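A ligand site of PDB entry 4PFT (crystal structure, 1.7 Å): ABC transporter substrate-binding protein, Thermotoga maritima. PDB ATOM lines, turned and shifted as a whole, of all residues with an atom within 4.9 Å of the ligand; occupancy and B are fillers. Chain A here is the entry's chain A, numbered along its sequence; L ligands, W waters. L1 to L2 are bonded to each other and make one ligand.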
ATOM      1  N   GLY A  13       5.100 -15.189   2.411  1.00  0.00           N
ATOM      2  CA  GLY A  13       4.624 -15.621   3.720  1.00  0.00           C
ATOM      3  C   GLY A  13       3.304 -14.956   4.057  1.00  0.00           C
ATOM      4  O   GLY A  13       2.594 -15.419   4.957  1.00  0.00           O
ATOM      5  N   ALA A  14       2.956 -13.893   3.325  1.00  0.00           N
ATOM      6  CA  ALA A  14       1.783 -13.093   3.641  1.00  0.00           C
ATOM      7  C   ALA A  14       0.723 -13.011   2.534  1.00  0.00           C
ATOM      8  O   ALA A  14      -0.308 -12.368   2.715  1.00  0.00           O
ATOM      9  CB  ALA A  14       2.232 -11.647   4.023  1.00  0.00           C
ATOM     10  N   LEU A  15       0.968 -13.673   1.396  1.00  0.00           N
ATOM     11  CA  LEU A  15       0.094 -13.559   0.234  1.00  0.00           C
ATOM     12  C   LEU A  15      -0.571 -14.910  -0.044  1.00  0.00           C
ATOM     13  O   LEU A  15       0.069 -15.819  -0.568  1.00  0.00           O
ATOM     14  CB  LEU A  15       0.882 -13.079  -0.986  1.00  0.00           C
ATOM     15  CG  LEU A  15       0.080 -12.731  -2.244  1.00  0.00           C
ATOM     16  CD1 LEU A  15      -0.936 -11.654  -1.887  1.00  0.00           C
ATOM     17  CD2 LEU A  15       0.979 -12.288  -3.400  1.00  0.00           C
ATOM     18  N   TRP A  16      -1.852 -15.039   0.330  1.00  0.00           N
ATOM     19  CA  TRP A  16      -2.525 -16.343   0.314  1.00  0.00           C
ATOM     20  C   TRP A  16      -3.805 -16.287  -0.498  1.00  0.00           C
ATOM     21  O   TRP A  16      -4.683 -17.148  -0.391  1.00  0.00           O
ATOM     22  CB  TRP A  16      -2.802 -16.796   1.757  1.00  0.00           C
ATOM     23  CG  TRP A  16      -1.525 -17.039   2.521  1.00  0.00           C
ATOM     24  CD1 TRP A  16      -0.890 -16.161   3.367  1.00  0.00           C
ATOM     25  CD2 TRP A  16      -0.697 -18.200   2.463  1.00  0.00           C
ATOM     26  NE1 TRP A  16       0.274 -16.744   3.862  1.00  0.00           N
ATOM     27  CE2 TRP A  16       0.402 -17.991   3.314  1.00  0.00           C
ATOM     28  CE3 TRP A  16      -0.798 -19.425   1.775  1.00  0.00           C
ATOM     29  CZ2 TRP A  16       1.412 -18.944   3.507  1.00  0.00           C
ATOM     30  CZ3 TRP A  16       0.200 -20.378   1.976  1.00  0.00           C
ATOM     31  CH2 TRP A  16       1.290 -20.136   2.839  1.00  0.00           C
ATOM     32  N   ASN A 212       3.017 -24.069   2.286  1.00  0.00           N
ATOM     33  CA  ASN A 212       4.350 -23.849   2.883  1.00  0.00           C
ATOM     34  C   ASN A 212       5.417 -24.749   2.256  1.00  0.00           C
ATOM     35  O   ASN A 212       6.583 -24.371   2.141  1.00  0.00           O
ATOM     36  CB  ASN A 212       4.326 -24.104   4.388  1.00  0.00           C
ATOM     37  CG  ASN A 212       3.532 -23.055   5.159  1.00  0.00           C
ATOM     38  OD1 ASN A 212       3.324 -21.948   4.687  1.00  0.00           O
ATOM     39  ND2 ASN A 212       3.108 -23.424   6.351  1.00  0.00           N
ATOM     40  N   ASN A 228       8.527 -15.342   5.427  1.00  0.00           N
ATOM     41  CA  ASN A 228       7.665 -15.315   6.602  1.00  0.00           C
ATOM     42  C   ASN A 228       6.658 -16.461   6.547  1.00  0.00           C
ATOM     43  O   ASN A 228       5.542 -16.357   7.067  1.00  0.00           O
ATOM     44  CB  ASN A 228       6.910 -13.979   6.728  1.00  0.00           C
ATOM     45  CG  ASN A 228       7.840 -12.804   7.011  1.00  0.00           C
ATOM     46  OD1 ASN A 228       7.697 -11.744   6.422  1.00  0.00           O
ATOM     47  ND2 ASN A 228       8.803 -13.006   7.912  1.00  0.00           N
ATOM     48  N   PHE A 229       7.085 -17.554   5.909  1.00  0.00           N
ATOM     49  CA  PHE A 229       6.371 -18.819   5.934  1.00  0.00           C
ATOM     50  C   PHE A 229       6.765 -19.597   7.164  1.00  0.00           C
ATOM     51  O   PHE A 229       7.928 -19.546   7.563  1.00  0.00           O
ATOM     52  CB  PHE A 229       6.725 -19.682   4.724  1.00  0.00           C
ATOM     53  CG  PHE A 229       6.316 -19.101   3.407  1.00  0.00           C
ATOM     54  CD1 PHE A 229       5.014 -19.249   2.925  1.00  0.00           C
ATOM     55  CD2 PHE A 229       7.255 -18.435   2.621  1.00  0.00           C
ATOM     56  CE1 PHE A 229       4.649 -18.731   1.702  1.00  0.00           C
ATOM     57  CE2 PHE A 229       6.908 -17.929   1.386  1.00  0.00           C
ATOM     58  CZ  PHE A 229       5.601 -18.060   0.921  1.00  0.00           C
ATOM     59  N   PHE A 230       5.850 -20.372   7.731  1.00  0.00           N
ATOM     60  CA  PHE A 230       6.328 -21.439   8.590  1.00  0.00           C
ATOM     61  C   PHE A 230       7.044 -22.484   7.725  1.00  0.00           C
ATOM     62  O   PHE A 230       6.482 -23.014   6.766  1.00  0.00           O
ATOM     63  CB  PHE A 230       5.208 -22.131   9.369  1.00  0.00           C
ATOM     64  CG  PHE A 230       5.669 -23.416  10.020  1.00  0.00           C
ATOM     65  CD1 PHE A 230       6.255 -23.401  11.264  1.00  0.00           C
ATOM     66  CD2 PHE A 230       5.562 -24.629   9.336  1.00  0.00           C
ATOM     67  CE1 PHE A 230       6.707 -24.584  11.835  1.00  0.00           C
ATOM     68  CE2 PHE A 230       6.016 -25.803   9.912  1.00  0.00           C
ATOM     69  CZ  PHE A 230       6.583 -25.781  11.154  1.00  0.00           C
ATOM     70  N   ASN A 257       2.228 -13.907  18.417  1.00  0.00           N
ATOM     71  CA  ASN A 257       0.822 -13.749  18.774  1.00  0.00           C
ATOM     72  C   ASN A 257       0.322 -14.954  19.537  1.00  0.00           C
ATOM     73  O   ASN A 257       1.058 -15.922  19.741  1.00  0.00           O
ATOM     74  CB  ASN A 257      -0.034 -13.571  17.520  1.00  0.00           C
ATOM     75  CG  ASN A 257       0.342 -14.560  16.428  1.00  0.00           C
ATOM     76  OD1 ASN A 257       0.248 -15.768  16.635  1.00  0.00           O
ATOM     77  ND2 ASN A 257       0.741 -14.051  15.279  1.00  0.00           N
ATOM     78  N   TYR A 293       5.646 -28.156  15.880  1.00  0.00           N
ATOM     79  CA  TYR A 293       6.636 -27.063  15.887  1.00  0.00           C
ATOM     80  C   TYR A 293       8.044 -27.463  16.314  1.00  0.00           C
ATOM     81  O   TYR A 293       8.959 -26.639  16.255  1.00  0.00           O
ATOM     82  CB  TYR A 293       6.129 -25.915  16.775  1.00  0.00           C
ATOM     83  CG  TYR A 293       4.887 -25.299  16.177  1.00  0.00           C
ATOM     84  CD1 TYR A 293       4.987 -24.534  15.028  1.00  0.00           C
ATOM     85  CD2 TYR A 293       3.626 -25.522  16.726  1.00  0.00           C
ATOM     86  CE1 TYR A 293       3.888 -23.991  14.430  1.00  0.00           C
ATOM     87  CE2 TYR A 293       2.496 -24.978  16.122  1.00  0.00           C
ATOM     88  CZ  TYR A 293       2.642 -24.230  14.976  1.00  0.00           C
ATOM     89  OH  TYR A 293       1.556 -23.688  14.347  1.00  0.00           O
ATOM     90  N   TRP A 368      -1.358 -24.154   5.160  1.00  0.00           N
ATOM     91  CA  TRP A 368      -0.685 -23.713   6.383  1.00  0.00           C
ATOM     92  C   TRP A 368      -0.325 -24.961   7.172  1.00  0.00           C
ATOM     93  O   TRP A 368      -1.048 -25.376   8.079  1.00  0.00           O
ATOM     94  CB  TRP A 368      -1.578 -22.773   7.208  1.00  0.00           C
ATOM     95  CG  TRP A 368      -1.749 -21.397   6.570  1.00  0.00           C
ATOM     96  CD1 TRP A 368      -1.519 -21.048   5.272  1.00  0.00           C
ATOM     97  CD2 TRP A 368      -2.169 -20.195   7.245  1.00  0.00           C
ATOM     98  NE1 TRP A 368      -1.785 -19.712   5.084  1.00  0.00           N
ATOM     99  CE2 TRP A 368      -2.174 -19.167   6.274  1.00  0.00           C
ATOM    100  CE3 TRP A 368      -2.517 -19.892   8.562  1.00  0.00           C
ATOM    101  CZ2 TRP A 368      -2.524 -17.865   6.585  1.00  0.00           C
ATOM    102  CZ3 TRP A 368      -2.866 -18.586   8.864  1.00  0.00           C
ATOM    103  CH2 TRP A 368      -2.870 -17.587   7.881  1.00  0.00           C
ATOM    104  N   THR A 369       0.774 -25.573   6.764  1.00  0.00           N
ATOM    105  CA  THR A 369       1.055 -26.953   7.147  1.00  0.00           C
ATOM    106  C   THR A 369       1.142 -27.198   8.648  1.00  0.00           C
ATOM    107  O   THR A 369       0.659 -28.234   9.132  1.00  0.00           O
ATOM    108  CB  THR A 369       2.354 -27.440   6.493  1.00  0.00           C
ATOM    109  OG1 THR A 369       3.423 -26.547   6.797  1.00  0.00           O
ATOM    110  CG2 THR A 369       2.154 -27.555   4.970  1.00  0.00           C
ATOM    111  N   ASP A 370       1.724 -26.250   9.390  1.00  0.00           N
ATOM    112  CA  ASP A 370       1.828 -26.373  10.846  1.00  0.00           C
ATOM    113  C   ASP A 370       0.460 -26.352  11.497  1.00  0.00           C
ATOM    114  O   ASP A 370       0.223 -27.021  12.502  1.00  0.00           O
ATOM    115  CB  ASP A 370       2.694 -25.263  11.442  1.00  0.00           C
ATOM    116  CG  ASP A 370       2.281 -23.877  10.977  1.00  0.00           C
ATOM    117  OD1 ASP A 370       1.993 -23.722   9.771  1.00  0.00           O
ATOM    118  OD2 ASP A 370       2.234 -22.937  11.822  1.00  0.00           O
ATOM    119  N   TRP A 371      -0.450 -25.561  10.925  1.00  0.00           N
ATOM    120  CA  TRP A 371      -1.768 -25.446  11.517  1.00  0.00           C
ATOM    121  C   TRP A 371      -2.624 -26.660  11.167  1.00  0.00           C
ATOM    122  O   TRP A 371      -3.476 -27.066  11.960  1.00  0.00           O
ATOM    123  CB  TRP A 371      -2.451 -24.143  11.101  1.00  0.00           C
ATOM    124  CG  TRP A 371      -2.023 -22.986  11.976  1.00  0.00           C
ATOM    125  CD1 TRP A 371      -0.930 -22.943  12.789  1.00  0.00           C
ATOM    126  CD2 TRP A 371      -2.707 -21.737  12.158  1.00  0.00           C
ATOM    127  NE1 TRP A 371      -0.879 -21.743  13.444  1.00  0.00           N
ATOM    128  CE2 TRP A 371      -1.952 -20.985  13.077  1.00  0.00           C
ATOM    129  CE3 TRP A 371      -3.871 -21.189  11.616  1.00  0.00           C
ATOM    130  CZ2 TRP A 371      -2.334 -19.694  13.477  1.00  0.00           C
ATOM    131  CZ3 TRP A 371      -4.238 -19.888  12.011  1.00  0.00           C
ATOM    132  CH2 TRP A 371      -3.474 -19.168  12.941  1.00  0.00           C
ATOM    133  N   ASN A 414      -5.191 -16.432  14.938  1.00  0.00           N
ATOM    134  CA  ASN A 414      -4.272 -15.583  15.690  1.00  0.00           C
ATOM    135  C   ASN A 414      -4.166 -14.142  15.129  1.00  0.00           C
ATOM    136  O   ASN A 414      -3.177 -13.469  15.366  1.00  0.00           O
ATOM    137  CB  ASN A 414      -2.889 -16.202  15.685  1.00  0.00           C
ATOM    138  CG  ASN A 414      -2.279 -16.190  14.304  1.00  0.00           C
ATOM    139  OD1 ASN A 414      -2.975 -15.914  13.327  1.00  0.00           O
ATOM    140  ND2 ASN A 414      -0.980 -16.450  14.201  1.00  0.00           N
ATOM    141  N   PHE A 415      -5.179 -13.678  14.394  1.00  0.00           N
ATOM    142  CA  PHE A 415      -5.069 -12.426  13.644  1.00  0.00           C
ATOM    143  C   PHE A 415      -5.024 -11.176  14.530  1.00  0.00           C
ATOM    144  O   PHE A 415      -4.381 -10.178  14.198  1.00  0.00           O
ATOM    145  CB  PHE A 415      -6.248 -12.267  12.676  1.00  0.00           C
ATOM    146  CG  PHE A 415      -6.180 -13.128  11.449  1.00  0.00           C
ATOM    147  CD1 PHE A 415      -5.102 -13.967  11.206  1.00  0.00           C
ATOM    148  CD2 PHE A 415      -7.219 -13.104  10.511  1.00  0.00           C
ATOM    149  CE1 PHE A 415      -5.075 -14.753  10.068  1.00  0.00           C
ATOM    150  CE2 PHE A 415      -7.184 -13.897   9.360  1.00  0.00           C
ATOM    151  CZ  PHE A 415      -6.113 -14.724   9.143  1.00  0.00           C
ATOM    152  N   ASN A 493       2.094 -18.487  18.599  1.00  0.00           N
ATOM    153  CA  ASN A 493       2.543 -18.810  17.251  1.00  0.00           C
ATOM    154  C   ASN A 493       3.818 -18.027  16.977  1.00  0.00           C
ATOM    155  O   ASN A 493       4.013 -16.970  17.537  1.00  0.00           O
ATOM    156  CB  ASN A 493       1.477 -18.477  16.206  1.00  0.00           C
ATOM    157  CG  ASN A 493       1.468 -19.474  15.047  1.00  0.00           C
ATOM    158  OD1 ASN A 493       1.458 -20.685  15.272  1.00  0.00           O
ATOM    159  ND2 ASN A 493       1.523 -18.981  13.817  1.00  0.00           N
ATOM    160  N   TRP A 496       7.379 -16.150  12.149  1.00  0.00           N
ATOM    161  CA  TRP A 496       8.176 -16.960  11.225  1.00  0.00           C
ATOM    162  C   TRP A 496       9.071 -16.077  10.411  1.00  0.00           C
ATOM    163  O   TRP A 496       8.612 -15.157   9.737  1.00  0.00           O
ATOM    164  CB  TRP A 496       7.282 -17.799  10.294  1.00  0.00           C
ATOM    165  CG  TRP A 496       6.215 -18.526  11.036  1.00  0.00           C
ATOM    166  CD1 TRP A 496       4.872 -18.463  10.791  1.00  0.00           C
ATOM    167  CD2 TRP A 496       6.382 -19.413  12.148  1.00  0.00           C
ATOM    168  NE1 TRP A 496       4.194 -19.268  11.697  1.00  0.00           N
ATOM    169  CE2 TRP A 496       5.102 -19.852  12.534  1.00  0.00           C
ATOM    170  CE3 TRP A 496       7.501 -19.883  12.870  1.00  0.00           C
ATOM    171  CZ2 TRP A 496       4.898 -20.737  13.598  1.00  0.00           C
ATOM    172  CZ3 TRP A 496       7.304 -20.752  13.920  1.00  0.00           C
ATOM    173  CH2 TRP A 496       6.010 -21.173  14.278  1.00  0.00           C
ATOM    174  N   TRP A 520       4.126  -9.491   7.352  1.00  0.00           N
ATOM    175  CA  TRP A 520       2.682  -9.703   7.422  1.00  0.00           C
ATOM    176  C   TRP A 520       2.003  -8.356   7.592  1.00  0.00           C
ATOM    177  O   TRP A 520       2.580  -7.442   8.196  1.00  0.00           O
ATOM    178  CB  TRP A 520       2.305 -10.601   8.609  1.00  0.00           C
ATOM    179  CG  TRP A 520       2.838 -11.976   8.551  1.00  0.00           C
ATOM    180  CD1 TRP A 520       3.052 -12.746   7.438  1.00  0.00           C
ATOM    181  CD2 TRP A 520       3.218 -12.780   9.678  1.00  0.00           C
ATOM    182  NE1 TRP A 520       3.539 -13.980   7.807  1.00  0.00           N
ATOM    183  CE2 TRP A 520       3.669 -14.019   9.171  1.00  0.00           C
ATOM    184  CE3 TRP A 520       3.247 -12.546  11.059  1.00  0.00           C
ATOM    185  CZ2 TRP A 520       4.116 -15.060  10.001  1.00  0.00           C
ATOM    186  CZ3 TRP A 520       3.698 -13.574  11.906  1.00  0.00           C
ATOM    187  CH2 TRP A 520       4.127 -14.820  11.359  1.00  0.00           C
ATOM    188  N   ASN A 521       0.789  -8.194   7.062  1.00  0.00           N
ATOM    189  CA  ASN A 521       0.037  -6.989   7.377  1.00  0.00           C
ATOM    190  C   ASN A 521      -0.025  -6.752   8.884  1.00  0.00           C
ATOM    191  O   ASN A 521      -0.287  -7.693   9.656  1.00  0.00           O
ATOM    192  CB  ASN A 521      -1.384  -7.042   6.810  1.00  0.00           C
ATOM    193  CG  ASN A 521      -2.178  -5.800   7.176  1.00  0.00           C
ATOM    194  OD1 ASN A 521      -1.778  -4.677   6.855  1.00  0.00           O
ATOM    195  ND2 ASN A 521      -3.285  -5.988   7.873  1.00  0.00           N
ATOM    196  N   TRP A 523       2.606  -5.618  10.565  1.00  0.00           N
ATOM    197  CA  TRP A 523       3.949  -5.718  11.116  1.00  0.00           C
ATOM    198  C   TRP A 523       4.962  -4.746  10.510  1.00  0.00           C
ATOM    199  O   TRP A 523       6.017  -4.497  11.103  1.00  0.00           O
ATOM    200  CB  TRP A 523       4.447  -7.167  10.996  1.00  0.00           C
ATOM    201  CG  TRP A 523       3.786  -8.086  11.979  1.00  0.00           C
ATOM    202  CD1 TRP A 523       2.537  -8.634  11.859  1.00  0.00           C
ATOM    203  CD2 TRP A 523       4.332  -8.573  13.222  1.00  0.00           C
ATOM    204  NE1 TRP A 523       2.269  -9.428  12.948  1.00  0.00           N
ATOM    205  CE2 TRP A 523       3.343  -9.401  13.806  1.00  0.00           C
ATOM    206  CE3 TRP A 523       5.538  -8.393  13.895  1.00  0.00           C
ATOM    207  CZ2 TRP A 523       3.554 -10.072  15.019  1.00  0.00           C
ATOM    208  CZ3 TRP A 523       5.745  -9.049  15.103  1.00  0.00           C
ATOM    209  CH2 TRP A 523       4.760  -9.870  15.647  1.00  0.00           C
HETATM  210  C1  LIG L   1      -0.690 -13.377  10.052  1.00  0.00           C
HETATM  211  C2  LIG L   1      -0.819 -14.469  11.056  1.00  0.00           C
HETATM  212  C3  LIG L   1       0.359 -15.233  10.523  1.00  0.00           C
HETATM  213  C4  LIG L   1       0.138 -15.592   9.057  1.00  0.00           C
HETATM  214  C5  LIG L   1      -0.175 -14.367   8.213  1.00  0.00           C
HETATM  215  C6  LIG L   1      -0.400 -14.653   6.745  1.00  0.00           C
HETATM  216  O1  LIG L   1      -0.550 -12.097  10.439  1.00  0.00           O
HETATM  217  O2  LIG L   1      -1.990 -15.273  10.878  1.00  0.00           O
HETATM  218  O3  LIG L   1       0.601 -16.393  11.335  1.00  0.00           O
HETATM  219  O4  LIG L   1       1.373 -16.195   8.561  1.00  0.00           O
HETATM  220  O5  LIG L   1      -1.334 -13.639   8.757  1.00  0.00           O
HETATM  221  O6  LIG L   1      -0.515 -13.425   6.012  1.00  0.00           O
HETATM  222  C1  LG2 L   2       1.151 -17.543   8.227  1.00  0.00           C
HETATM  223  C2  LG2 L   2       2.289 -18.064   7.378  1.00  0.00           C
HETATM  224  C3  LG2 L   2       2.139 -19.548   7.124  1.00  0.00           C
HETATM  225  C4  LG2 L   2       1.959 -20.338   8.400  1.00  0.00           C
HETATM  226  C5  LG2 L   2       0.804 -19.730   9.204  1.00  0.00           C
HETATM  227  C6  LG2 L   2       0.509 -20.422  10.508  1.00  0.00           C
HETATM  228  O1  LG2 L   2       3.526 -17.767   8.098  1.00  0.00           O
HETATM  229  O2  LG2 L   2       3.327 -20.028   6.415  1.00  0.00           O
HETATM  230  O3  LG2 L   2       1.657 -21.699   8.076  1.00  0.00           O
HETATM  231  O4  LG2 L   2       1.050 -18.325   9.479  1.00  0.00           O
HETATM  232  O5  LG2 L   2       1.660 -20.448  11.348  1.00  0.00           O
HETATM  233  O   HOH W   1      -0.693 -10.585   6.339  1.00  0.00           O
HETATM  234  O   HOH W   2       2.180 -16.099  13.691  1.00  0.00           O
HETATM  235  O   HOH W   3       0.378 -11.526  13.070  1.00  0.00           O
HETATM  236  O   HOH W   4      -1.376 -10.210   9.099  1.00  0.00           O
HETATM  237  O   HOH W   5      -3.251 -10.532  11.623  1.00  0.00           O
HETATM  238  O   HOH W   6      -2.841 -13.010   4.536  1.00  0.00           O
HETATM  239  O   HOH W   7      -3.646 -12.659   7.569  1.00  0.00           O
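O of Gly 13 touches C6 of LIG L1, at 3.6 Å. NE1 of Trp 16 touches C6 of LIG L1 (3.6 Å). Phe 229 touches the ligand. CE3 of Trp 368 touches C5 of LG2 L2, at 3.4 Å. NE1 of Trp 371 touches C6 of LG2 L2 (3.5 Å). Phe 415 touches the ligand. Of the 21 residues printed, 15 come within 4 Å of the ligand.
Water W4 bridges an oxygen (O1) of LIG L1 (2.5 Å) and the backbone carbonyl oxygen (O) of Asn 521 (2.8 Å). Water W6 bridges O6 of LIG L1 (2.8 Å) and O of Ala 14 (3.2 Å). Water W3 lies within hydrogen-bond range of the indole nitrogen (NE1) of Trp 523 (2.8 Å), an oxygen (O1) of LIG L1 (2.8 Å) and the side-chain amide nitrogen (ND2) of Asn 257 (3.4 Å). Water W1 lies within hydrogen-bond range of an oxygen (O6) of LIG L1 (2.9 Å) and the backbone NH of Asn 521 (2.9 Å). Water W5 lies within hydrogen-bond range of O of Phe 415 and O1 of LIG L1.
The side-chain amide nitrogen (ND2) of Asn 212 lies close to the backbone carbonyl oxygen (O) of Phe 230 (3.4 Å). The side-chain amide oxygen (OD1) of Asn 493 sits at hydrogen-bond distance from the indole nitrogen (NE1) of Trp 371 (3.2 Å). OD2 of Asp 370 lies within hydrogen-bond range of OH of Tyr 293, at 2.7 Å. The indole nitrogen (NE1) of Trp 371 sits close to the side-chain hydroxyl (OH) of Tyr 293 (3.2 Å). The backbone carbonyl oxygen of Asn 228 is in hydrogen-bond range of the indole nitrogen of Trp 520, at 3.2 Å. OH of Tyr 293 is in hydrogen-bond range of OD1 of Asn 493 (3.1 Å). The indole nitrogen (NE1) of Trp 520 sits at hydrogen-bond distance from the backbone carbonyl oxygen (O) of Gly 13, 3.3 Å away. NE1 of Trp 496 sits close to ND2 of Asn 493 (3.4 Å).
The side-chain amide oxygen (OD1) of Asn 414 is in hydrogen-bond range of an oxygen (O2) of LIG L1, 2.7 Å away. O1 of LG2 L2 lies within hydrogen-bond range of O of Asn 228, 2.7 Å away. An oxygen (O5) of LG2 L2 sits at hydrogen-bond distance from the side-chain carboxylate (OD2) of Asp 370, at 2.6 Å. An oxygen (O5) of LG2 L2 lies within hydrogen-bond range of the side-chain amide nitrogen (ND2) of Asn 493 (2.9 Å). The indole nitrogen (NE1) of Trp 520 lies within hydrogen-bond range of an oxygen (O4) of LIG L1 (3.2 Å). O2 of LG2 L2 sits at hydrogen-bond distance from OD1 of Asn 212, at 2.6 Å. The backbone carbonyl oxygen of Ala 14 sits close to an oxygen (O6) of LIG L1, at 3.5 Å. The backbone NH (N) of Phe 230 lies within hydrogen-bond range of an oxygen (O2) of LG2 L2, at 2.9 Å. NE1 of Trp 496 sits at hydrogen-bond distance from O5 of LG2 L2 (2.8 Å).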
